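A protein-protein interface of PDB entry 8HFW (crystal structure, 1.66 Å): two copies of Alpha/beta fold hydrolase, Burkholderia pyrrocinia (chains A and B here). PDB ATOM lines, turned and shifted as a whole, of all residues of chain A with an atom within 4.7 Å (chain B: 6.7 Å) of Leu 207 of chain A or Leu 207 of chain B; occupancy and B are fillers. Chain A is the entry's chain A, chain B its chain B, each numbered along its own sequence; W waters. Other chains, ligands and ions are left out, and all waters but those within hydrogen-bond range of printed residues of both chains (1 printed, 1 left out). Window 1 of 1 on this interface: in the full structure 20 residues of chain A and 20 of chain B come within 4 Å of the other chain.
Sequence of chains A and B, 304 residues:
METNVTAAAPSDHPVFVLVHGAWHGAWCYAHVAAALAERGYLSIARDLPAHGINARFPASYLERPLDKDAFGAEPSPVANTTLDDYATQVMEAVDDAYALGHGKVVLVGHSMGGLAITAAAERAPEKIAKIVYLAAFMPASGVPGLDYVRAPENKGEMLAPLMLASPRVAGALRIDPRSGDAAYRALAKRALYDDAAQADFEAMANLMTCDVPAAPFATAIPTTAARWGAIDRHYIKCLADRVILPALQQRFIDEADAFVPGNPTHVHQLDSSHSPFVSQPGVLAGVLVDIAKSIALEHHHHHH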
ATOM      1  N   TRP A  27     -21.378  11.663   1.881  1.00  0.00           N
ATOM      2  CA  TRP A  27     -22.817  11.641   2.122  1.00  0.00           C
ATOM      3  C   TRP A  27     -23.423  13.034   2.248  1.00  0.00           C
ATOM      4  O   TRP A  27     -24.633  13.177   2.091  1.00  0.00           O
ATOM      5  CB  TRP A  27     -23.137  10.816   3.377  1.00  0.00           C
ATOM      6  CG  TRP A  27     -22.238  11.038   4.550  1.00  0.00           C
ATOM      7  CD1 TRP A  27     -21.173  10.271   4.906  1.00  0.00           C
ATOM      8  CD2 TRP A  27     -22.303  12.098   5.523  1.00  0.00           C
ATOM      9  NE1 TRP A  27     -20.577  10.772   6.029  1.00  0.00           N
ATOM     10  CE2 TRP A  27     -21.236  11.900   6.416  1.00  0.00           C
ATOM     11  CE3 TRP A  27     -23.144  13.201   5.711  1.00  0.00           C
ATOM     12  CZ2 TRP A  27     -21.002  12.751   7.492  1.00  0.00           C
ATOM     13  CZ3 TRP A  27     -22.924  14.038   6.790  1.00  0.00           C
ATOM     14  CH2 TRP A  27     -21.855  13.816   7.644  1.00  0.00           C
ATOM     15  N   GLY A  52     -15.417   9.120   6.796  1.00  0.00           N
ATOM     16  CA  GLY A  52     -16.405   8.220   6.223  1.00  0.00           C
ATOM     17  C   GLY A  52     -16.041   6.748   6.416  1.00  0.00           C
ATOM     18  O   GLY A  52     -15.838   6.296   7.536  1.00  0.00           O
ATOM     19  N   ILE A  53     -16.046   6.003   5.305  1.00  0.00           N
ATOM     20  CA  ILE A  53     -15.689   4.594   5.306  1.00  0.00           C
ATOM     21  C   ILE A  53     -14.215   4.401   5.662  1.00  0.00           C
ATOM     22  O   ILE A  53     -13.826   3.281   5.986  1.00  0.00           O
ATOM     23  CB  ILE A  53     -16.042   3.976   3.938  1.00  0.00           C
ATOM     24  CG1 ILE A  53     -15.171   4.520   2.792  1.00  0.00           C
ATOM     25  CG2 ILE A  53     -17.544   4.127   3.675  1.00  0.00           C
ATOM     26  N   ALA A 203     -29.774  13.460  11.304  1.00  0.00           N
ATOM     27  CA  ALA A 203     -29.325  12.452  10.340  1.00  0.00           C
ATOM     28  C   ALA A 203     -27.856  12.679   9.956  1.00  0.00           C
ATOM     29  O   ALA A 203     -27.089  11.741   9.848  1.00  0.00           O
ATOM     30  CB  ALA A 203     -30.247  12.471   9.138  1.00  0.00           C
ATOM     31  N   MET A 204     -27.452  13.954   9.782  1.00  0.00           N
ATOM     32  CA  MET A 204     -26.070  14.279   9.460  1.00  0.00           C
ATOM     33  C   MET A 204     -25.173  13.971  10.662  1.00  0.00           C
ATOM     34  O   MET A 204     -24.073  13.454  10.521  1.00  0.00           O
ATOM     35  CB  MET A 204     -25.908  15.758   9.091  1.00  0.00           C
ATOM     36  CG  MET A 204     -26.753  16.180   7.893  1.00  0.00           C
ATOM     37  SD  MET A 204     -26.314  15.383   6.354  1.00  0.00           S
ATOM     38  N   ALA A 205     -25.620  14.354  11.850  1.00  0.00           N
ATOM     39  CA  ALA A 205     -24.814  14.156  13.035  1.00  0.00           C
ATOM     40  C   ALA A 205     -24.550  12.672  13.245  1.00  0.00           C
ATOM     41  O   ALA A 205     -23.534  12.324  13.812  1.00  0.00           O
ATOM     42  CB  ALA A 205     -25.508  14.755  14.223  1.00  0.00           C
ATOM     43  N   ASN A 206     -25.503  11.801  12.886  1.00  0.00           N
ATOM     44  CA  ASN A 206     -25.321  10.361  12.993  1.00  0.00           C
ATOM     45  C   ASN A 206     -24.169   9.869  12.102  1.00  0.00           C
ATOM     46  O   ASN A 206     -23.540   8.879  12.443  1.00  0.00           O
ATOM     47  CB  ASN A 206     -26.602   9.619  12.605  1.00  0.00           C
ATOM     48  CG  ASN A 206     -26.446   8.111  12.530  1.00  0.00           C
ATOM     49  OD1 ASN A 206     -26.420   7.498  11.442  1.00  0.00           O
ATOM     50  ND2 ASN A 206     -26.243   7.516  13.692  1.00  0.00           N
ATOM     51  N   LEU A 207     -23.932  10.512  10.947  1.00  0.00           N
ATOM     52  CA  LEU A 207     -22.933  10.050   9.995  1.00  0.00           C
ATOM     53  C   LEU A 207     -21.563  10.671  10.256  1.00  0.00           C
ATOM     54  O   LEU A 207     -20.575  10.160   9.776  1.00  0.00           O
ATOM     55  CB  LEU A 207     -23.415  10.362   8.579  1.00  0.00           C
ATOM     56  CG  LEU A 207     -24.744   9.723   8.171  1.00  0.00           C
ATOM     57  CD1 LEU A 207     -25.247  10.286   6.878  1.00  0.00           C
ATOM     58  CD2 LEU A 207     -24.637   8.212   8.070  1.00  0.00           C
ATOM     59  N   MET A 208     -21.520  11.777  11.001  1.00  0.00           N
ATOM     60  CA  MET A 208     -20.270  12.449  11.309  1.00  0.00           C
ATOM     61  C   MET A 208     -19.356  11.545  12.127  1.00  0.00           C
ATOM     62  O   MET A 208     -19.831  10.621  12.813  1.00  0.00           O
ATOM     63  CB  MET A 208     -20.542  13.726  12.106  1.00  0.00           C
ATOM     64  CG  MET A 208     -21.121  14.824  11.229  1.00  0.00           C
ATOM     65  SD  MET A 208     -21.666  16.261  12.182  1.00  0.00           S
ATOM     66  CE  MET A 208     -20.087  16.881  12.727  1.00  0.00           C
ATOM     67  N   THR A 209     -18.034  11.788  12.032  1.00  0.00           N
ATOM     68  CA  THR A 209     -17.014  11.100  12.820  1.00  0.00           C
ATOM     69  C   THR A 209     -16.459  12.087  13.850  1.00  0.00           C
ATOM     70  O   THR A 209     -16.893  13.240  13.818  1.00  0.00           O
ATOM     71  CB  THR A 209     -15.936  10.526  11.904  1.00  0.00           C
ATOM     72  OG1 THR A 209     -15.378  11.567  11.111  1.00  0.00           O
ATOM     73  CG2 THR A 209     -16.488   9.448  10.980  1.00  0.00           C
ATOM     74  N   TRP B  23     -30.840  -0.720   7.303  1.00  0.00           N
ATOM     75  CA  TRP B  23     -29.939  -0.067   8.256  1.00  0.00           C
ATOM     76  C   TRP B  23     -28.701   0.530   7.591  1.00  0.00           C
ATOM     77  O   TRP B  23     -27.879   1.092   8.305  1.00  0.00           O
ATOM     78  CB  TRP B  23     -29.496  -1.024   9.382  1.00  0.00           C
ATOM     79  CG  TRP B  23     -30.643  -1.590  10.161  1.00  0.00           C
ATOM     80  CD1 TRP B  23     -31.522  -0.916  10.949  1.00  0.00           C
ATOM     81  CD2 TRP B  23     -31.039  -2.969  10.210  1.00  0.00           C
ATOM     82  NE1 TRP B  23     -32.441  -1.780  11.498  1.00  0.00           N
ATOM     83  CE2 TRP B  23     -32.161  -3.051  11.066  1.00  0.00           C
ATOM     84  CE3 TRP B  23     -30.543  -4.133   9.620  1.00  0.00           C
ATOM     85  CZ2 TRP B  23     -32.809  -4.259  11.321  1.00  0.00           C
ATOM     86  CZ3 TRP B  23     -31.152  -5.333   9.912  1.00  0.00           C
ATOM     87  CH2 TRP B  23     -32.275  -5.390  10.741  1.00  0.00           C
ATOM     88  N   HIS B  24     -28.565   0.394   6.258  1.00  0.00           N
ATOM     89  CA  HIS B  24     -27.374   0.866   5.562  1.00  0.00           C
ATOM     90  C   HIS B  24     -27.738   2.113   4.759  1.00  0.00           C
ATOM     91  O   HIS B  24     -28.814   2.640   4.922  1.00  0.00           O
ATOM     92  CB  HIS B  24     -26.772  -0.276   4.739  1.00  0.00           C
ATOM     93  CG  HIS B  24     -26.172  -1.352   5.595  1.00  0.00           C
ATOM     94  ND1 HIS B  24     -24.911  -1.863   5.385  1.00  0.00           N
ATOM     95  CD2 HIS B  24     -26.662  -1.977   6.691  1.00  0.00           C
ATOM     96  CE1 HIS B  24     -24.682  -2.778   6.310  1.00  0.00           C
ATOM     97  NE2 HIS B  24     -25.728  -2.862   7.102  1.00  0.00           N
ATOM     98  N   GLY B  25     -26.803   2.573   3.928  1.00  0.00           N
ATOM     99  CA  GLY B  25     -26.980   3.721   3.060  1.00  0.00           C
ATOM    100  C   GLY B  25     -26.161   3.541   1.796  1.00  0.00           C
ATOM    101  O   GLY B  25     -25.503   2.528   1.664  1.00  0.00           O
ATOM    102  N   TRP B  27     -23.510   4.897   1.029  1.00  0.00           N
ATOM    103  CA  TRP B  27     -22.107   4.848   1.412  1.00  0.00           C
ATOM    104  C   TRP B  27     -21.520   3.437   1.351  1.00  0.00           C
ATOM    105  O   TRP B  27     -20.309   3.301   1.216  1.00  0.00           O
ATOM    106  CB  TRP B  27     -21.918   5.462   2.811  1.00  0.00           C
ATOM    107  CG  TRP B  27     -22.902   4.974   3.832  1.00  0.00           C
ATOM    108  CD1 TRP B  27     -24.033   5.623   4.227  1.00  0.00           C
ATOM    109  CD2 TRP B  27     -22.855   3.753   4.605  1.00  0.00           C
ATOM    110  NE1 TRP B  27     -24.706   4.888   5.158  1.00  0.00           N
ATOM    111  CE2 TRP B  27     -24.013   3.741   5.418  1.00  0.00           C
ATOM    112  CE3 TRP B  27     -21.969   2.674   4.685  1.00  0.00           C
ATOM    113  CZ2 TRP B  27     -24.295   2.692   6.285  1.00  0.00           C
ATOM    114  CZ3 TRP B  27     -22.261   1.626   5.538  1.00  0.00           C
ATOM    115  CH2 TRP B  27     -23.389   1.667   6.325  1.00  0.00           C
ATOM    116  N   CYS B  28     -22.352   2.403   1.515  1.00  0.00           N
ATOM    117  CA  CYS B  28     -21.878   1.031   1.529  1.00  0.00           C
ATOM    118  C   CYS B  28     -21.306   0.635   0.161  1.00  0.00           C
ATOM    119  O   CYS B  28     -20.460  -0.241   0.100  1.00  0.00           O
ATOM    120  CB  CYS B  28     -22.983   0.069   1.986  1.00  0.00           C
ATOM    121  SG  CYS B  28     -24.205  -0.349   0.725  1.00  0.00           S
ATOM    122  N   ASP B  47     -29.584   6.990  -0.889  1.00  0.00           N
ATOM    123  CA  ASP B  47     -30.218   6.480   0.312  1.00  0.00           C
ATOM    124  C   ASP B  47     -31.703   6.213   0.056  1.00  0.00           C
ATOM    125  O   ASP B  47     -32.376   7.042  -0.534  1.00  0.00           O
ATOM    126  CB  ASP B  47     -30.099   7.472   1.463  1.00  0.00           C
ATOM    127  CG  ASP B  47     -28.674   7.743   1.909  1.00  0.00           C
ATOM    128  OD1 ASP B  47     -27.921   6.803   1.872  1.00  0.00           O
ATOM    129  OD2 ASP B  47     -28.338   8.848   2.377  1.00  0.00           O
ATOM    130  N   GLY B  52     -29.917   6.548   5.825  1.00  0.00           N
ATOM    131  CA  GLY B  52     -28.870   7.526   5.534  1.00  0.00           C
ATOM    132  C   GLY B  52     -29.292   8.936   5.930  1.00  0.00           C
ATOM    133  O   GLY B  52     -29.667   9.161   7.074  1.00  0.00           O
ATOM    134  N   ILE B  53     -29.200   9.875   4.980  1.00  0.00           N
ATOM    135  CA  ILE B  53     -29.548  11.266   5.223  1.00  0.00           C
ATOM    136  C   ILE B  53     -31.053  11.416   5.498  1.00  0.00           C
ATOM    137  O   ILE B  53     -31.474  12.481   5.934  1.00  0.00           O
ATOM    138  CB  ILE B  53     -29.086  12.135   4.031  1.00  0.00           C
ATOM    139  CG1 ILE B  53     -29.830  11.792   2.723  1.00  0.00           C
ATOM    140  CG2 ILE B  53     -27.574  12.034   3.918  1.00  0.00           C
ATOM    141  N   PHE B  57     -34.420   8.715  14.330  1.00  0.00           N
ATOM    142  CA  PHE B  57     -34.055   7.824  15.419  1.00  0.00           C
ATOM    143  C   PHE B  57     -35.026   7.984  16.580  1.00  0.00           C
ATOM    144  O   PHE B  57     -35.467   9.091  16.871  1.00  0.00           O
ATOM    145  CB  PHE B  57     -32.633   8.130  15.906  1.00  0.00           C
ATOM    146  CG  PHE B  57     -31.651   8.209  14.766  1.00  0.00           C
ATOM    147  CD1 PHE B  57     -30.924   7.104  14.381  1.00  0.00           C
ATOM    148  CD2 PHE B  57     -31.486   9.388  14.068  1.00  0.00           C
ATOM    149  CE1 PHE B  57     -30.058   7.164  13.313  1.00  0.00           C
ATOM    150  CE2 PHE B  57     -30.604   9.447  13.000  1.00  0.00           C
ATOM    151  CZ  PHE B  57     -29.899   8.341  12.622  1.00  0.00           C
ATOM    152  N   PRO B 177     -26.272  -0.439  16.104  1.00  0.00           N
ATOM    153  CA  PRO B 177     -24.915  -0.398  15.561  1.00  0.00           C
ATOM    154  C   PRO B 177     -23.983   0.469  16.408  1.00  0.00           C
ATOM    155  O   PRO B 177     -22.789   0.369  16.246  1.00  0.00           O
ATOM    156  CB  PRO B 177     -25.092   0.171  14.145  1.00  0.00           C
ATOM    157  CG  PRO B 177     -26.429   0.896  14.201  1.00  0.00           C
ATOM    158  CD  PRO B 177     -27.268   0.213  15.255  1.00  0.00           C
ATOM    159  N   GLU B 202     -15.812  -1.217  11.724  1.00  0.00           N
ATOM    160  CA  GLU B 202     -16.145  -0.143  12.656  1.00  0.00           C
ATOM    161  C   GLU B 202     -16.605   1.115  11.904  1.00  0.00           C
ATOM    162  O   GLU B 202     -17.490   1.814  12.373  1.00  0.00           O
ATOM    163  CB  GLU B 202     -14.943   0.210  13.538  1.00  0.00           C
ATOM    164  CG  GLU B 202     -14.587  -0.872  14.560  1.00  0.00           C
ATOM    165  CD  GLU B 202     -15.744  -1.263  15.469  1.00  0.00           C
ATOM    166  N   ALA B 203     -15.983   1.408  10.749  1.00  0.00           N
ATOM    167  CA  ALA B 203     -16.326   2.593   9.974  1.00  0.00           C
ATOM    168  C   ALA B 203     -17.715   2.442   9.373  1.00  0.00           C
ATOM    169  O   ALA B 203     -18.494   3.390   9.359  1.00  0.00           O
ATOM    170  CB  ALA B 203     -15.266   2.847   8.922  1.00  0.00           C
ATOM    171  N   MET B 204     -18.047   1.221   8.931  1.00  0.00           N
ATOM    172  CA  MET B 204     -19.365   0.938   8.365  1.00  0.00           C
ATOM    173  C   MET B 204     -20.442   0.958   9.457  1.00  0.00           C
ATOM    174  O   MET B 204     -21.522   1.520   9.247  1.00  0.00           O
ATOM    175  CB  MET B 204     -19.386  -0.411   7.633  1.00  0.00           C
ATOM    176  CG  MET B 204     -18.424  -0.504   6.492  1.00  0.00           C
ATOM    177  SD  MET B 204     -18.898   0.515   5.061  1.00  0.00           S
ATOM    178  N   ALA B 205     -20.131   0.361  10.617  1.00  0.00           N
ATOM    179  CA  ALA B 205     -21.074   0.298  11.722  1.00  0.00           C
ATOM    180  C   ALA B 205     -21.378   1.712  12.214  1.00  0.00           C
ATOM    181  O   ALA B 205     -22.504   1.960  12.611  1.00  0.00           O
ATOM    182  CB  ALA B 205     -20.518  -0.575  12.812  1.00  0.00           C
ATOM    183  N   ASN B 206     -20.394   2.644  12.133  1.00  0.00           N
ATOM    184  CA  ASN B 206     -20.627   4.027  12.516  1.00  0.00           C
ATOM    185  C   ASN B 206     -21.689   4.662  11.610  1.00  0.00           C
ATOM    186  O   ASN B 206     -22.393   5.534  12.076  1.00  0.00           O
ATOM    187  CB  ASN B 206     -19.358   4.881  12.484  1.00  0.00           C
ATOM    188  CG  ASN B 206     -19.615   6.327  12.840  1.00  0.00           C
ATOM    189  OD1 ASN B 206     -19.887   6.646  13.998  1.00  0.00           O
ATOM    190  ND2 ASN B 206     -19.501   7.208  11.855  1.00  0.00           N
ATOM    191  N   LEU B 207     -21.794   4.259  10.336  1.00  0.00           N
ATOM    192  CA  LEU B 207     -22.701   4.933   9.424  1.00  0.00           C
ATOM    193  C   LEU B 207     -24.089   4.304   9.459  1.00  0.00           C
ATOM    194  O   LEU B 207     -25.038   4.923   8.980  1.00  0.00           O
ATOM    195  CB  LEU B 207     -22.104   4.902   8.018  1.00  0.00           C
ATOM    196  CG  LEU B 207     -20.748   5.597   7.885  1.00  0.00           C
ATOM    197  CD1 LEU B 207     -20.104   5.275   6.548  1.00  0.00           C
ATOM    198  CD2 LEU B 207     -20.913   7.110   8.074  1.00  0.00           C
ATOM    199  N   MET B 208     -24.209   3.094  10.036  1.00  0.00           N
ATOM    200  CA  MET B 208     -25.476   2.384  10.013  1.00  0.00           C
ATOM    201  C   MET B 208     -26.498   3.099  10.916  1.00  0.00           C
ATOM    202  O   MET B 208     -26.116   3.883  11.797  1.00  0.00           O
ATOM    203  CB  MET B 208     -25.308   0.932  10.503  1.00  0.00           C
ATOM    204  CG  MET B 208     -24.700   0.004   9.479  1.00  0.00           C
ATOM    205  SD  MET B 208     -24.242  -1.592  10.206  1.00  0.00           S
ATOM    206  CE  MET B 208     -25.883  -2.280  10.462  1.00  0.00           C
ATOM    207  N   THR B 209     -27.800   2.841  10.690  1.00  0.00           N
ATOM    208  CA  THR B 209     -28.909   3.403  11.456  1.00  0.00           C
ATOM    209  C   THR B 209     -29.582   2.284  12.248  1.00  0.00           C
ATOM    210  O   THR B 209     -29.176   1.129  12.098  1.00  0.00           O
ATOM    211  CB  THR B 209     -29.907   4.125  10.529  1.00  0.00           C
ATOM    212  OG1 THR B 209     -30.375   3.227   9.529  1.00  0.00           O
ATOM    213  CG2 THR B 209     -29.285   5.366   9.881  1.00  0.00           C
HETATM  214  O   HOH W   1     -17.591   5.933   9.710  1.00  0.00           O
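NE2 of His 24 of chain B lies close to SD of Met 208 of chain B (3.7 Å).
The backbone NH of Ile 53 of chain B lies within hydrogen-bond range of the side-chain carboxylate of Asp 47 of chain B, 2.9 Å away.
The backbone carbonyl oxygen (O) of Trp 23 of chain B sits at hydrogen-bond distance from the backbone NH (N) of Thr 209 of chain B.
Among the printed residues, merely in contact across the chains: Ile 53 of chain A with Ala 203 of chain B (3.3 Å), Ala 203 of chain A with Ile 53 of chain B (3.4 Å), Leu 207 of chain A with Leu 207 of chain B (3.4 Å), Asn 206 of chain A with Phe 57 of chain B (3.5 Å), Asn 206 of chain A with Asn 206 of chain B (3.6 Å), Met 208 of chain A with Asn 206 of chain B (3.6 Å), Asn 206 of chain A with Met 208 of chain B (3.6 Å), Trp 27 of chain A with Ile 53 of chain B (3.6 Å), Gly 52 of chain A with Ala 203 of chain B (3.8 Å), Leu 207 of chain A with Asn 206 of chain B (3.8 Å), Ile 53 of chain A with Trp 27 of chain B (3.8 Å), Asn 206 of chain A with Leu 207 of chain B (3.8 Å), Thr 209 of chain A with Asn 206 of chain B (3.9 Å), Asn 206 of chain A with Thr 209 of chain B (3.9 Å) and Ala 203 of chain A with Gly 52 of chain B (3.9 Å).
Of the printed residues of chain B, Ile 53 of chain A touches Trp 27 (3.8 Å) and Ala 203 (3.3 Å).
Of the printed residues of chain B, Asn 206 of chain A touches Phe 57 (3.5 Å), Asn 206 (3.6 Å), Leu 207 (3.8 Å), Met 208 (3.6 Å) and Thr 209 (3.9 Å).
Of chain B, only Asn 206 (3.8 Å) and Leu 207 (3.4 Å) come within 4 Å of Leu 207 of chain A.
Printed residues of chain A within 4 Å of Gly 52 of chain B: Ala 203.
Of the printed residues of chain A, Leu 207 of chain B touches Asn 206 and Leu 207.
Printed residues of chain A within 4 Å of Met 208 of chain B: Asn 206 (3.6 Å).
Of the printed residues of chain A, Thr 209 of chain B touches Asn 206 (3.9 Å).
The nearest printed residue of chain A that does not touch Leu 207 of chain B is Ile 53 of chain A (4.02 Å).
The nearest printed residue of chain B that does not touch Asn 206 of chain A is Gly 52 of chain B (5.7 Å).
Ile 53 of chain A touches Ala 203 of chain B, and with the chains exchanged Ala 203 of chain A touches Ile 53 of chain B.
Asn 206 of chain B touches its own counterpart, Asn 206 of chain A.
Asn 206 of chain A touches Met 208 of chain B, and with the chains exchanged Met 208 of chain A touches Asn 206 of chain B.
Asn 206 of chain A touches Thr 209 of chain B, and with the chains exchanged Thr 209 of chain A touches Asn 206 of chain B.
10 positions are printed for both chains.
Water W1 lies within hydrogen-bond range of O of Ala 203 of chain B (2.7 Å), O of Gly 52 of chain A (2.8 Å) and ND2 of Asn 206 of chain B (3.1 Å).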
